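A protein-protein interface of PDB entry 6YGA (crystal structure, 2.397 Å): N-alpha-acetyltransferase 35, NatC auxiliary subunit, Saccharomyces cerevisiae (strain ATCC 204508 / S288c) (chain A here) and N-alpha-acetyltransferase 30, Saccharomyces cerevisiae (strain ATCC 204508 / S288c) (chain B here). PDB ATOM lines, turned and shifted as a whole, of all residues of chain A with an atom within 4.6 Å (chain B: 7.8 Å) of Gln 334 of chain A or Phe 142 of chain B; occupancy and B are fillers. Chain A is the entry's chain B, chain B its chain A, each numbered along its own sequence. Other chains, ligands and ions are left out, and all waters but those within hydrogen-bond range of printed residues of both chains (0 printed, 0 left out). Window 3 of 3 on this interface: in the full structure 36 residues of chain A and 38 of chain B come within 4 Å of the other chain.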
ATOM      1  N   TYR A 107     -28.934 -21.065  13.083  1.00  0.00           N
ATOM      2  CA  TYR A 107     -28.639 -22.111  14.069  1.00  0.00           C
ATOM      3  C   TYR A 107     -29.891 -22.885  14.484  1.00  0.00           C
ATOM      4  O   TYR A 107     -30.036 -23.286  15.642  1.00  0.00           O
ATOM      5  CB  TYR A 107     -27.945 -21.527  15.304  1.00  0.00           C
ATOM      6  CG  TYR A 107     -26.734 -20.670  15.009  1.00  0.00           C
ATOM      7  CD1 TYR A 107     -25.478 -21.240  14.855  1.00  0.00           C
ATOM      8  CD2 TYR A 107     -26.844 -19.288  14.907  1.00  0.00           C
ATOM      9  CE1 TYR A 107     -24.365 -20.461  14.593  1.00  0.00           C
ATOM     10  CE2 TYR A 107     -25.737 -18.499  14.644  1.00  0.00           C
ATOM     11  CZ  TYR A 107     -24.500 -19.091  14.489  1.00  0.00           C
ATOM     12  OH  TYR A 107     -23.396 -18.312  14.227  1.00  0.00           O
ATOM     13  N   GLU A 175     -23.977 -26.702  18.667  1.00  0.00           N
ATOM     14  CA  GLU A 175     -23.676 -25.390  19.224  1.00  0.00           C
ATOM     15  C   GLU A 175     -23.444 -24.437  18.064  1.00  0.00           C
ATOM     16  O   GLU A 175     -24.155 -23.437  17.913  1.00  0.00           O
ATOM     17  CB  GLU A 175     -22.460 -25.453  20.156  1.00  0.00           C
ATOM     18  CG  GLU A 175     -22.041 -24.110  20.752  1.00  0.00           C
ATOM     19  CD  GLU A 175     -20.767 -24.199  21.581  1.00  0.00           C
ATOM     20  OE1 GLU A 175     -20.246 -25.319  21.760  1.00  0.00           O
ATOM     21  OE2 GLU A 175     -20.286 -23.147  22.052  1.00  0.00           O
ATOM     22  N   ASP A 176     -22.461 -24.759  17.225  1.00  0.00           N
ATOM     23  CA  ASP A 176     -22.241 -24.011  15.996  1.00  0.00           C
ATOM     24  C   ASP A 176     -23.138 -24.500  14.871  1.00  0.00           C
ATOM     25  O   ASP A 176     -23.484 -23.722  13.974  1.00  0.00           O
ATOM     26  CB  ASP A 176     -20.778 -24.122  15.577  1.00  0.00           C
ATOM     27  CG  ASP A 176     -19.838 -23.630  16.647  1.00  0.00           C
ATOM     28  OD1 ASP A 176     -20.022 -22.485  17.109  1.00  0.00           O
ATOM     29  OD2 ASP A 176     -18.933 -24.393  17.041  1.00  0.00           O
ATOM     30  N   ASN A 330     -11.783 -13.631  11.482  1.00  0.00           N
ATOM     31  CA  ASN A 330     -12.944 -14.013  12.277  1.00  0.00           C
ATOM     32  C   ASN A 330     -13.068 -13.152  13.528  1.00  0.00           C
ATOM     33  O   ASN A 330     -13.673 -13.575  14.516  1.00  0.00           O
ATOM     34  CB  ASN A 330     -12.851 -15.496  12.647  1.00  0.00           C
ATOM     35  CG  ASN A 330     -14.173 -16.076  13.115  1.00  0.00           C
ATOM     36  OD1 ASN A 330     -15.239 -15.659  12.666  1.00  0.00           O
ATOM     37  ND2 ASN A 330     -14.108 -17.032  14.034  1.00  0.00           N
ATOM     38  N   GLU A 333     -16.475  -9.810  13.402  1.00  0.00           N
ATOM     39  CA  GLU A 333     -17.754 -10.453  13.660  1.00  0.00           C
ATOM     40  C   GLU A 333     -17.627 -11.932  13.334  1.00  0.00           C
ATOM     41  O   GLU A 333     -16.755 -12.346  12.564  1.00  0.00           O
ATOM     42  CB  GLU A 333     -18.895  -9.809  12.860  1.00  0.00           C
ATOM     43  CG  GLU A 333     -18.788  -9.982  11.356  1.00  0.00           C
ATOM     44  CD  GLU A 333     -19.928  -9.313  10.610  1.00  0.00           C
ATOM     45  OE1 GLU A 333     -20.678  -8.534  11.235  1.00  0.00           O
ATOM     46  OE2 GLU A 333     -20.074  -9.567   9.396  1.00  0.00           O
ATOM     47  N   GLN A 334     -18.507 -12.727  13.935  1.00  0.00           N
ATOM     48  CA  GLN A 334     -18.433 -14.174  13.793  1.00  0.00           C
ATOM     49  C   GLN A 334     -18.791 -14.591  12.371  1.00  0.00           C
ATOM     50  O   GLN A 334     -19.862 -14.248  11.863  1.00  0.00           O
ATOM     51  CB  GLN A 334     -19.365 -14.846  14.800  1.00  0.00           C
ATOM     52  CG  GLN A 334     -19.306 -16.364  14.792  1.00  0.00           C
ATOM     53  CD  GLN A 334     -19.990 -16.979  15.998  1.00  0.00           C
ATOM     54  OE1 GLN A 334     -19.822 -16.515  17.125  1.00  0.00           O
ATOM     55  NE2 GLN A 334     -20.771 -18.026  15.763  1.00  0.00           N
ATOM     56  N   ARG A 335     -17.892 -15.335  11.732  1.00  0.00           N
ATOM     57  CA  ARG A 335     -18.105 -15.779  10.362  1.00  0.00           C
ATOM     58  C   ARG A 335     -19.130 -16.907  10.310  1.00  0.00           C
ATOM     59  O   ARG A 335     -19.420 -17.572  11.308  1.00  0.00           O
ATOM     60  CB  ARG A 335     -16.791 -16.252   9.736  1.00  0.00           C
ATOM     61  CG  ARG A 335     -15.764 -15.155   9.505  1.00  0.00           C
ATOM     62  CD  ARG A 335     -16.181 -14.226   8.375  1.00  0.00           C
ATOM     63  NE  ARG A 335     -15.160 -13.220   8.093  1.00  0.00           N
ATOM     64  CZ  ARG A 335     -15.241 -12.326   7.112  1.00  0.00           C
ATOM     65  NH1 ARG A 335     -16.300 -12.308   6.312  1.00  0.00           N
ATOM     66  NH2 ARG A 335     -14.264 -11.448   6.931  1.00  0.00           N
ATOM     67  N   HIS A 336     -19.678 -17.120   9.113  1.00  0.00           N
ATOM     68  CA  HIS A 336     -20.607 -18.217   8.887  1.00  0.00           C
ATOM     69  C   HIS A 336     -19.958 -19.541   9.277  1.00  0.00           C
ATOM     70  O   HIS A 336     -18.748 -19.734   9.114  1.00  0.00           O
ATOM     71  CB  HIS A 336     -21.039 -18.230   7.418  1.00  0.00           C
ATOM     72  CG  HIS A 336     -22.237 -19.081   7.141  1.00  0.00           C
ATOM     73  ND1 HIS A 336     -22.162 -20.450   7.003  1.00  0.00           N
ATOM     74  CD2 HIS A 336     -23.541 -18.756   6.965  1.00  0.00           C
ATOM     75  CE1 HIS A 336     -23.367 -20.934   6.759  1.00  0.00           C
ATOM     76  NE2 HIS A 336     -24.221 -19.927   6.731  1.00  0.00           N
ATOM     77  N   ARG A 340     -16.278 -21.213   8.807  1.00  0.00           N
ATOM     78  CA  ARG A 340     -15.438 -21.470   9.972  1.00  0.00           C
ATOM     79  C   ARG A 340     -14.970 -22.920  10.012  1.00  0.00           C
ATOM     80  O   ARG A 340     -13.862 -23.205  10.475  1.00  0.00           O
ATOM     81  CB  ARG A 340     -16.180 -21.098  11.254  1.00  0.00           C
ATOM     82  CG  ARG A 340     -16.400 -19.603  11.400  1.00  0.00           C
ATOM     83  CD  ARG A 340     -16.794 -19.202  12.811  1.00  0.00           C
ATOM     84  NE  ARG A 340     -18.146 -19.627  13.160  1.00  0.00           N
ATOM     85  CZ  ARG A 340     -18.428 -20.621  13.996  1.00  0.00           C
ATOM     86  NH1 ARG A 340     -17.448 -21.302  14.576  1.00  0.00           N
ATOM     87  NH2 ARG A 340     -19.691 -20.930  14.257  1.00  0.00           N
ATOM     88  N   ASN A 405     -16.376 -20.150  17.591  1.00  0.00           N
ATOM     89  CA  ASN A 405     -17.307 -19.069  17.876  1.00  0.00           C
ATOM     90  C   ASN A 405     -16.754 -18.177  18.988  1.00  0.00           C
ATOM     91  O   ASN A 405     -15.739 -18.479  19.622  1.00  0.00           O
ATOM     92  CB  ASN A 405     -18.694 -19.611  18.238  1.00  0.00           C
ATOM     93  CG  ASN A 405     -18.708 -20.406  19.533  1.00  0.00           C
ATOM     94  OD1 ASN A 405     -18.534 -19.854  20.621  1.00  0.00           O
ATOM     95  ND2 ASN A 405     -18.951 -21.707  19.422  1.00  0.00           N
ATOM     96  N   THR A 406     -17.448 -17.061  19.223  1.00  0.00           N
ATOM     97  CA  THR A 406     -16.912 -16.010  20.084  1.00  0.00           C
ATOM     98  C   THR A 406     -16.752 -16.453  21.535  1.00  0.00           C
ATOM     99  O   THR A 406     -15.937 -15.870  22.258  1.00  0.00           O
ATOM    100  CB  THR A 406     -17.798 -14.761  20.002  1.00  0.00           C
ATOM    101  OG1 THR A 406     -17.141 -13.667  20.655  1.00  0.00           O
ATOM    102  CG2 THR A 406     -19.145 -15.006  20.666  1.00  0.00           C
ATOM    103  N   CYS A 407     -17.492 -17.472  21.974  1.00  0.00           N
ATOM    104  CA  CYS A 407     -17.321 -18.013  23.317  1.00  0.00           C
ATOM    105  C   CYS A 407     -16.248 -19.096  23.363  1.00  0.00           C
ATOM    106  O   CYS A 407     -15.382 -19.076  24.243  1.00  0.00           O
ATOM    107  CB  CYS A 407     -18.649 -18.566  23.836  1.00  0.00           C
ATOM    108  SG  CYS A 407     -19.897 -17.307  24.150  1.00  0.00           S
ATOM    109  N   LYS B 139     -17.564 -18.405  32.892  1.00  0.00           N
ATOM    110  CA  LYS B 139     -17.655 -18.980  31.559  1.00  0.00           C
ATOM    111  C   LYS B 139     -18.913 -18.463  30.880  1.00  0.00           C
ATOM    112  O   LYS B 139     -19.910 -18.167  31.544  1.00  0.00           O
ATOM    113  CB  LYS B 139     -17.676 -20.512  31.630  1.00  0.00           C
ATOM    114  CG  LYS B 139     -17.396 -21.232  30.324  1.00  0.00           C
ATOM    115  CD  LYS B 139     -17.393 -22.738  30.556  1.00  0.00           C
ATOM    116  CE  LYS B 139     -16.837 -23.504  29.372  1.00  0.00           C
ATOM    117  NZ  LYS B 139     -16.755 -24.958  29.670  1.00  0.00           N
ATOM    118  N   ARG B 140     -18.854 -18.359  29.556  1.00  0.00           N
ATOM    119  CA  ARG B 140     -20.009 -18.017  28.737  1.00  0.00           C
ATOM    120  C   ARG B 140     -20.191 -19.098  27.685  1.00  0.00           C
ATOM    121  O   ARG B 140     -19.246 -19.425  26.959  1.00  0.00           O
ATOM    122  CB  ARG B 140     -19.845 -16.650  28.067  1.00  0.00           C
ATOM    123  CG  ARG B 140     -21.125 -16.111  27.437  1.00  0.00           C
ATOM    124  CD  ARG B 140     -20.857 -14.830  26.657  1.00  0.00           C
ATOM    125  NE  ARG B 140     -22.040 -14.336  25.954  1.00  0.00           N
ATOM    126  CZ  ARG B 140     -22.691 -13.220  26.271  1.00  0.00           C
ATOM    127  NH1 ARG B 140     -22.275 -12.469  27.282  1.00  0.00           N
ATOM    128  NH2 ARG B 140     -23.757 -12.852  25.573  1.00  0.00           N
ATOM    129  N   MET B 141     -21.393 -19.657  27.608  1.00  0.00           N
ATOM    130  CA  MET B 141     -21.653 -20.766  26.695  1.00  0.00           C
ATOM    131  C   MET B 141     -22.531 -20.330  25.526  1.00  0.00           C
ATOM    132  O   MET B 141     -23.648 -19.854  25.719  1.00  0.00           O
ATOM    133  CB  MET B 141     -22.296 -21.937  27.443  1.00  0.00           C
ATOM    134  CG  MET B 141     -21.412 -22.527  28.534  1.00  0.00           C
ATOM    135  SD  MET B 141     -21.455 -21.524  30.209  1.00  0.00           S
ATOM    136  CE  MET B 141     -22.733 -22.621  31.189  1.00  0.00           C
ATOM    137  N   PHE B 142     -22.009 -20.506  24.314  1.00  0.00           N
ATOM    138  CA  PHE B 142     -22.656 -20.006  23.107  1.00  0.00           C
ATOM    139  C   PHE B 142     -23.962 -20.752  22.841  1.00  0.00           C
ATOM    140  O   PHE B 142     -23.961 -21.976  22.665  1.00  0.00           O
ATOM    141  CB  PHE B 142     -21.700 -20.144  21.926  1.00  0.00           C
ATOM    142  CG  PHE B 142     -22.257 -19.655  20.620  1.00  0.00           C
ATOM    143  CD1 PHE B 142     -22.294 -18.301  20.330  1.00  0.00           C
ATOM    144  CD2 PHE B 142     -22.719 -20.553  19.672  1.00  0.00           C
ATOM    145  CE1 PHE B 142     -22.800 -17.851  19.126  1.00  0.00           C
ATOM    146  CE2 PHE B 142     -23.221 -20.111  18.466  1.00  0.00           C
ATOM    147  CZ  PHE B 142     -23.264 -18.757  18.192  1.00  0.00           C
ATOM    148  N   ARG B 143     -25.070 -20.004  22.815  1.00  0.00           N
ATOM    149  CA  ARG B 143     -26.401 -20.538  22.504  1.00  0.00           C
ATOM    150  C   ARG B 143     -26.753 -21.727  23.397  1.00  0.00           C
ATOM    151  O   ARG B 143     -27.378 -22.696  22.963  1.00  0.00           O
ATOM    152  CB  ARG B 143     -26.515 -20.903  21.022  1.00  0.00           C
ATOM    153  CG  ARG B 143     -26.450 -19.701  20.093  1.00  0.00           C
ATOM    154  CD  ARG B 143     -26.720 -20.084  18.647  1.00  0.00           C
ATOM    155  NE  ARG B 143     -28.029 -20.707  18.485  1.00  0.00           N
ATOM    156  CZ  ARG B 143     -29.164 -20.031  18.341  1.00  0.00           C
ATOM    157  NH1 ARG B 143     -29.151 -18.707  18.343  1.00  0.00           N
ATOM    158  NH2 ARG B 143     -30.311 -20.679  18.199  1.00  0.00           N
ATOM    159  N   TYR B 144     -26.340 -21.641  24.663  1.00  0.00           N
ATOM    160  CA  TYR B 144     -26.629 -22.699  25.626  1.00  0.00           C
ATOM    161  C   TYR B 144     -28.130 -22.880  25.809  1.00  0.00           C
ATOM    162  O   TYR B 144     -28.609 -24.003  26.009  1.00  0.00           O
ATOM    163  CB  TYR B 144     -25.947 -22.366  26.952  1.00  0.00           C
ATOM    164  CG  TYR B 144     -26.036 -23.431  28.020  1.00  0.00           C
ATOM    165  CD1 TYR B 144     -25.085 -24.442  28.102  1.00  0.00           C
ATOM    166  CD2 TYR B 144     -27.050 -23.408  28.966  1.00  0.00           C
ATOM    167  CE1 TYR B 144     -25.154 -25.411  29.087  1.00  0.00           C
ATOM    168  CE2 TYR B 144     -27.130 -24.370  29.951  1.00  0.00           C
ATOM    169  CZ  TYR B 144     -26.179 -25.369  30.009  1.00  0.00           C
ATOM    170  OH  TYR B 144     -26.260 -26.327  30.992  1.00  0.00           O
ATOM    171  N   TYR B 145     -28.890 -21.787  25.741  1.00  0.00           N
ATOM    172  CA  TYR B 145     -30.344 -21.829  25.824  1.00  0.00           C
ATOM    173  C   TYR B 145     -31.005 -21.670  24.460  1.00  0.00           C
ATOM    174  O   TYR B 145     -32.122 -21.152  24.370  1.00  0.00           O
ATOM    175  CB  TYR B 145     -30.856 -20.762  26.794  1.00  0.00           C
ATOM    176  CG  TYR B 145     -30.420 -20.995  28.222  1.00  0.00           C
ATOM    177  CD1 TYR B 145     -30.999 -21.999  28.988  1.00  0.00           C
ATOM    178  CD2 TYR B 145     -29.427 -20.217  28.804  1.00  0.00           C
ATOM    179  CE1 TYR B 145     -30.602 -22.224  30.291  1.00  0.00           C
ATOM    180  CE2 TYR B 145     -29.025 -20.433  30.109  1.00  0.00           C
ATOM    181  CZ  TYR B 145     -29.615 -21.439  30.848  1.00  0.00           C
ATOM    182  OH  TYR B 145     -29.224 -21.668  32.147  1.00  0.00           O
ATOM    183  N   LEU B 146     -30.325 -22.101  23.396  1.00  0.00           N
ATOM    184  CA  LEU B 146     -30.883 -22.160  22.041  1.00  0.00           C
ATOM    185  C   LEU B 146     -31.310 -20.755  21.633  1.00  0.00           C
ATOM    186  O   LEU B 146     -30.468 -19.840  21.666  1.00  0.00           O
ATOM    187  CB  LEU B 146     -31.984 -23.221  22.026  1.00  0.00           C
ATOM    188  CG  LEU B 146     -31.610 -24.573  22.638  1.00  0.00           C
ATOM    189  CD1 LEU B 146     -32.857 -25.349  23.034  1.00  0.00           C
ATOM    190  CD2 LEU B 146     -30.757 -25.378  21.669  1.00  0.00           C
ATOM    191  N   GLY B 149     -30.662 -17.566  23.971  1.00  0.00           N
ATOM    192  CA  GLY B 149     -29.369 -16.915  24.048  1.00  0.00           C
ATOM    193  C   GLY B 149     -28.334 -17.739  24.796  1.00  0.00           C
ATOM    194  O   GLY B 149     -28.518 -18.922  25.096  1.00  0.00           O
ATOM    195  N   ASP B 150     -27.222 -17.076  25.098  1.00  0.00           N
ATOM    196  CA  ASP B 150     -26.085 -17.711  25.743  1.00  0.00           C
ATOM    197  C   ASP B 150     -26.359 -17.924  27.231  1.00  0.00           C
ATOM    198  O   ASP B 150     -27.387 -17.511  27.776  1.00  0.00           O
ATOM    199  CB  ASP B 150     -24.826 -16.867  25.546  1.00  0.00           C
ATOM    200  CG  ASP B 150     -24.519 -16.605  24.081  1.00  0.00           C
ATOM    201  OD1 ASP B 150     -25.169 -17.225  23.214  1.00  0.00           O
ATOM    202  OD2 ASP B 150     -23.624 -15.776  23.800  1.00  0.00           O
ATOM    203  N   ALA B 151     -25.414 -18.577  27.901  1.00  0.00           N
ATOM    204  CA  ALA B 151     -25.475 -18.773  29.338  1.00  0.00           C
ATOM    205  C   ALA B 151     -24.194 -18.263  29.974  1.00  0.00           C
ATOM    206  O   ALA B 151     -23.148 -18.162  29.328  1.00  0.00           O
ATOM    207  CB  ALA B 151     -25.660 -20.245  29.716  1.00  0.00           C
ATOM    208  N   PHE B 152     -24.300 -17.935  31.254  1.00  0.00           N
ATOM    209  CA  PHE B 152     -23.151 -17.706  32.115  1.00  0.00           C
ATOM    210  C   PHE B 152     -23.031 -18.878  33.078  1.00  0.00           C
ATOM    211  O   PHE B 152     -24.041 -19.402  33.563  1.00  0.00           O
ATOM    212  CB  PHE B 152     -23.284 -16.397  32.904  1.00  0.00           C
ATOM    213  CG  PHE B 152     -22.969 -15.157  32.108  1.00  0.00           C
ATOM    214  CD1 PHE B 152     -21.933 -15.150  31.190  1.00  0.00           C
ATOM    215  CD2 PHE B 152     -23.706 -13.994  32.287  1.00  0.00           C
ATOM    216  CE1 PHE B 152     -21.640 -14.007  30.463  1.00  0.00           C
ATOM    217  CE2 PHE B 152     -23.418 -12.848  31.561  1.00  0.00           C
ATOM    218  CZ  PHE B 152     -22.386 -12.855  30.650  1.00  0.00           C
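The backbone carbonyl oxygen (O) of Arg 140 of chain B sits close to the side-chain sulfur (SG) of Cys 407 of chain A (3.6 Å).
The backbone NH (N) of Arg 143 of chain B is in hydrogen-bond range of the side-chain carboxylate (OD1) of Asp 150 of chain B (2.8 Å).
The side-chain carboxylate (OE2) of Glu 175 of chain A lies within hydrogen-bond range of the side-chain amide nitrogen (ND2) of Asn 405 of chain A (3.3 Å).
The side-chain carboxylate of Asp 176 of chain A sits at hydrogen-bond distance from the side-chain amide nitrogen of Asn 405 of chain A (2.7 Å).
The guanidinium group (NH2) of Arg 340 of chain A lies close to the side-chain amide nitrogen (NE2) of Gln 334 of chain A.
The backbone NH (N) of Thr 406 of chain A lies within hydrogen-bond range of the side-chain amide oxygen (OE1) of Gln 334 of chain A, at 3.2 Å.
The side-chain amide oxygen (OD1) of Asn 405 of chain A is in hydrogen-bond range of the backbone NH (N) of Cys 407 of chain A (2.9 Å).
Among the printed residues, merely in contact across the chains: Tyr 107 of chain A with Arg 143 of chain B, Glu 175 of chain A with Phe 142 of chain B, Asn 405 of chain A with Phe 142 of chain B, Gln 334 of chain A with Phe 142 of chain B, Cys 407 of chain A with Phe 142 of chain B and Tyr 107 of chain A with Phe 142 of chain B.
Gln 334 of chain A touches one residue of chain B.
Of chain A, only Tyr 107, Glu 175, Gln 334, Asn 405 and Cys 407 come within 4 Å of Phe 142 of chain B.
Of the printed residues of chain B, Asn 405 of chain A touches Phe 142 (3.4 Å).
Of the printed residues of chain B, Tyr 107 of chain A touches Phe 142 (3.9 Å) and Arg 143 (3.3 Å).
The nearest residue of chain B that does not touch Gln 334 of chain A is Arg 143 of chain B (6.9 Å).
The nearest printed residue of chain B that does not touch Asn 405 of chain A is Met 141 of chain B (6.3 Å).
Of the 12 printed residues of chain A, 5 touch a printed residue of chain B.
Hydrophobic or aromatic side chains of chain A within 4 Å of the printed part of chain B: Tyr 107.
Of the 12 printed residues of chain B, 3 touch a printed residue of chain A.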
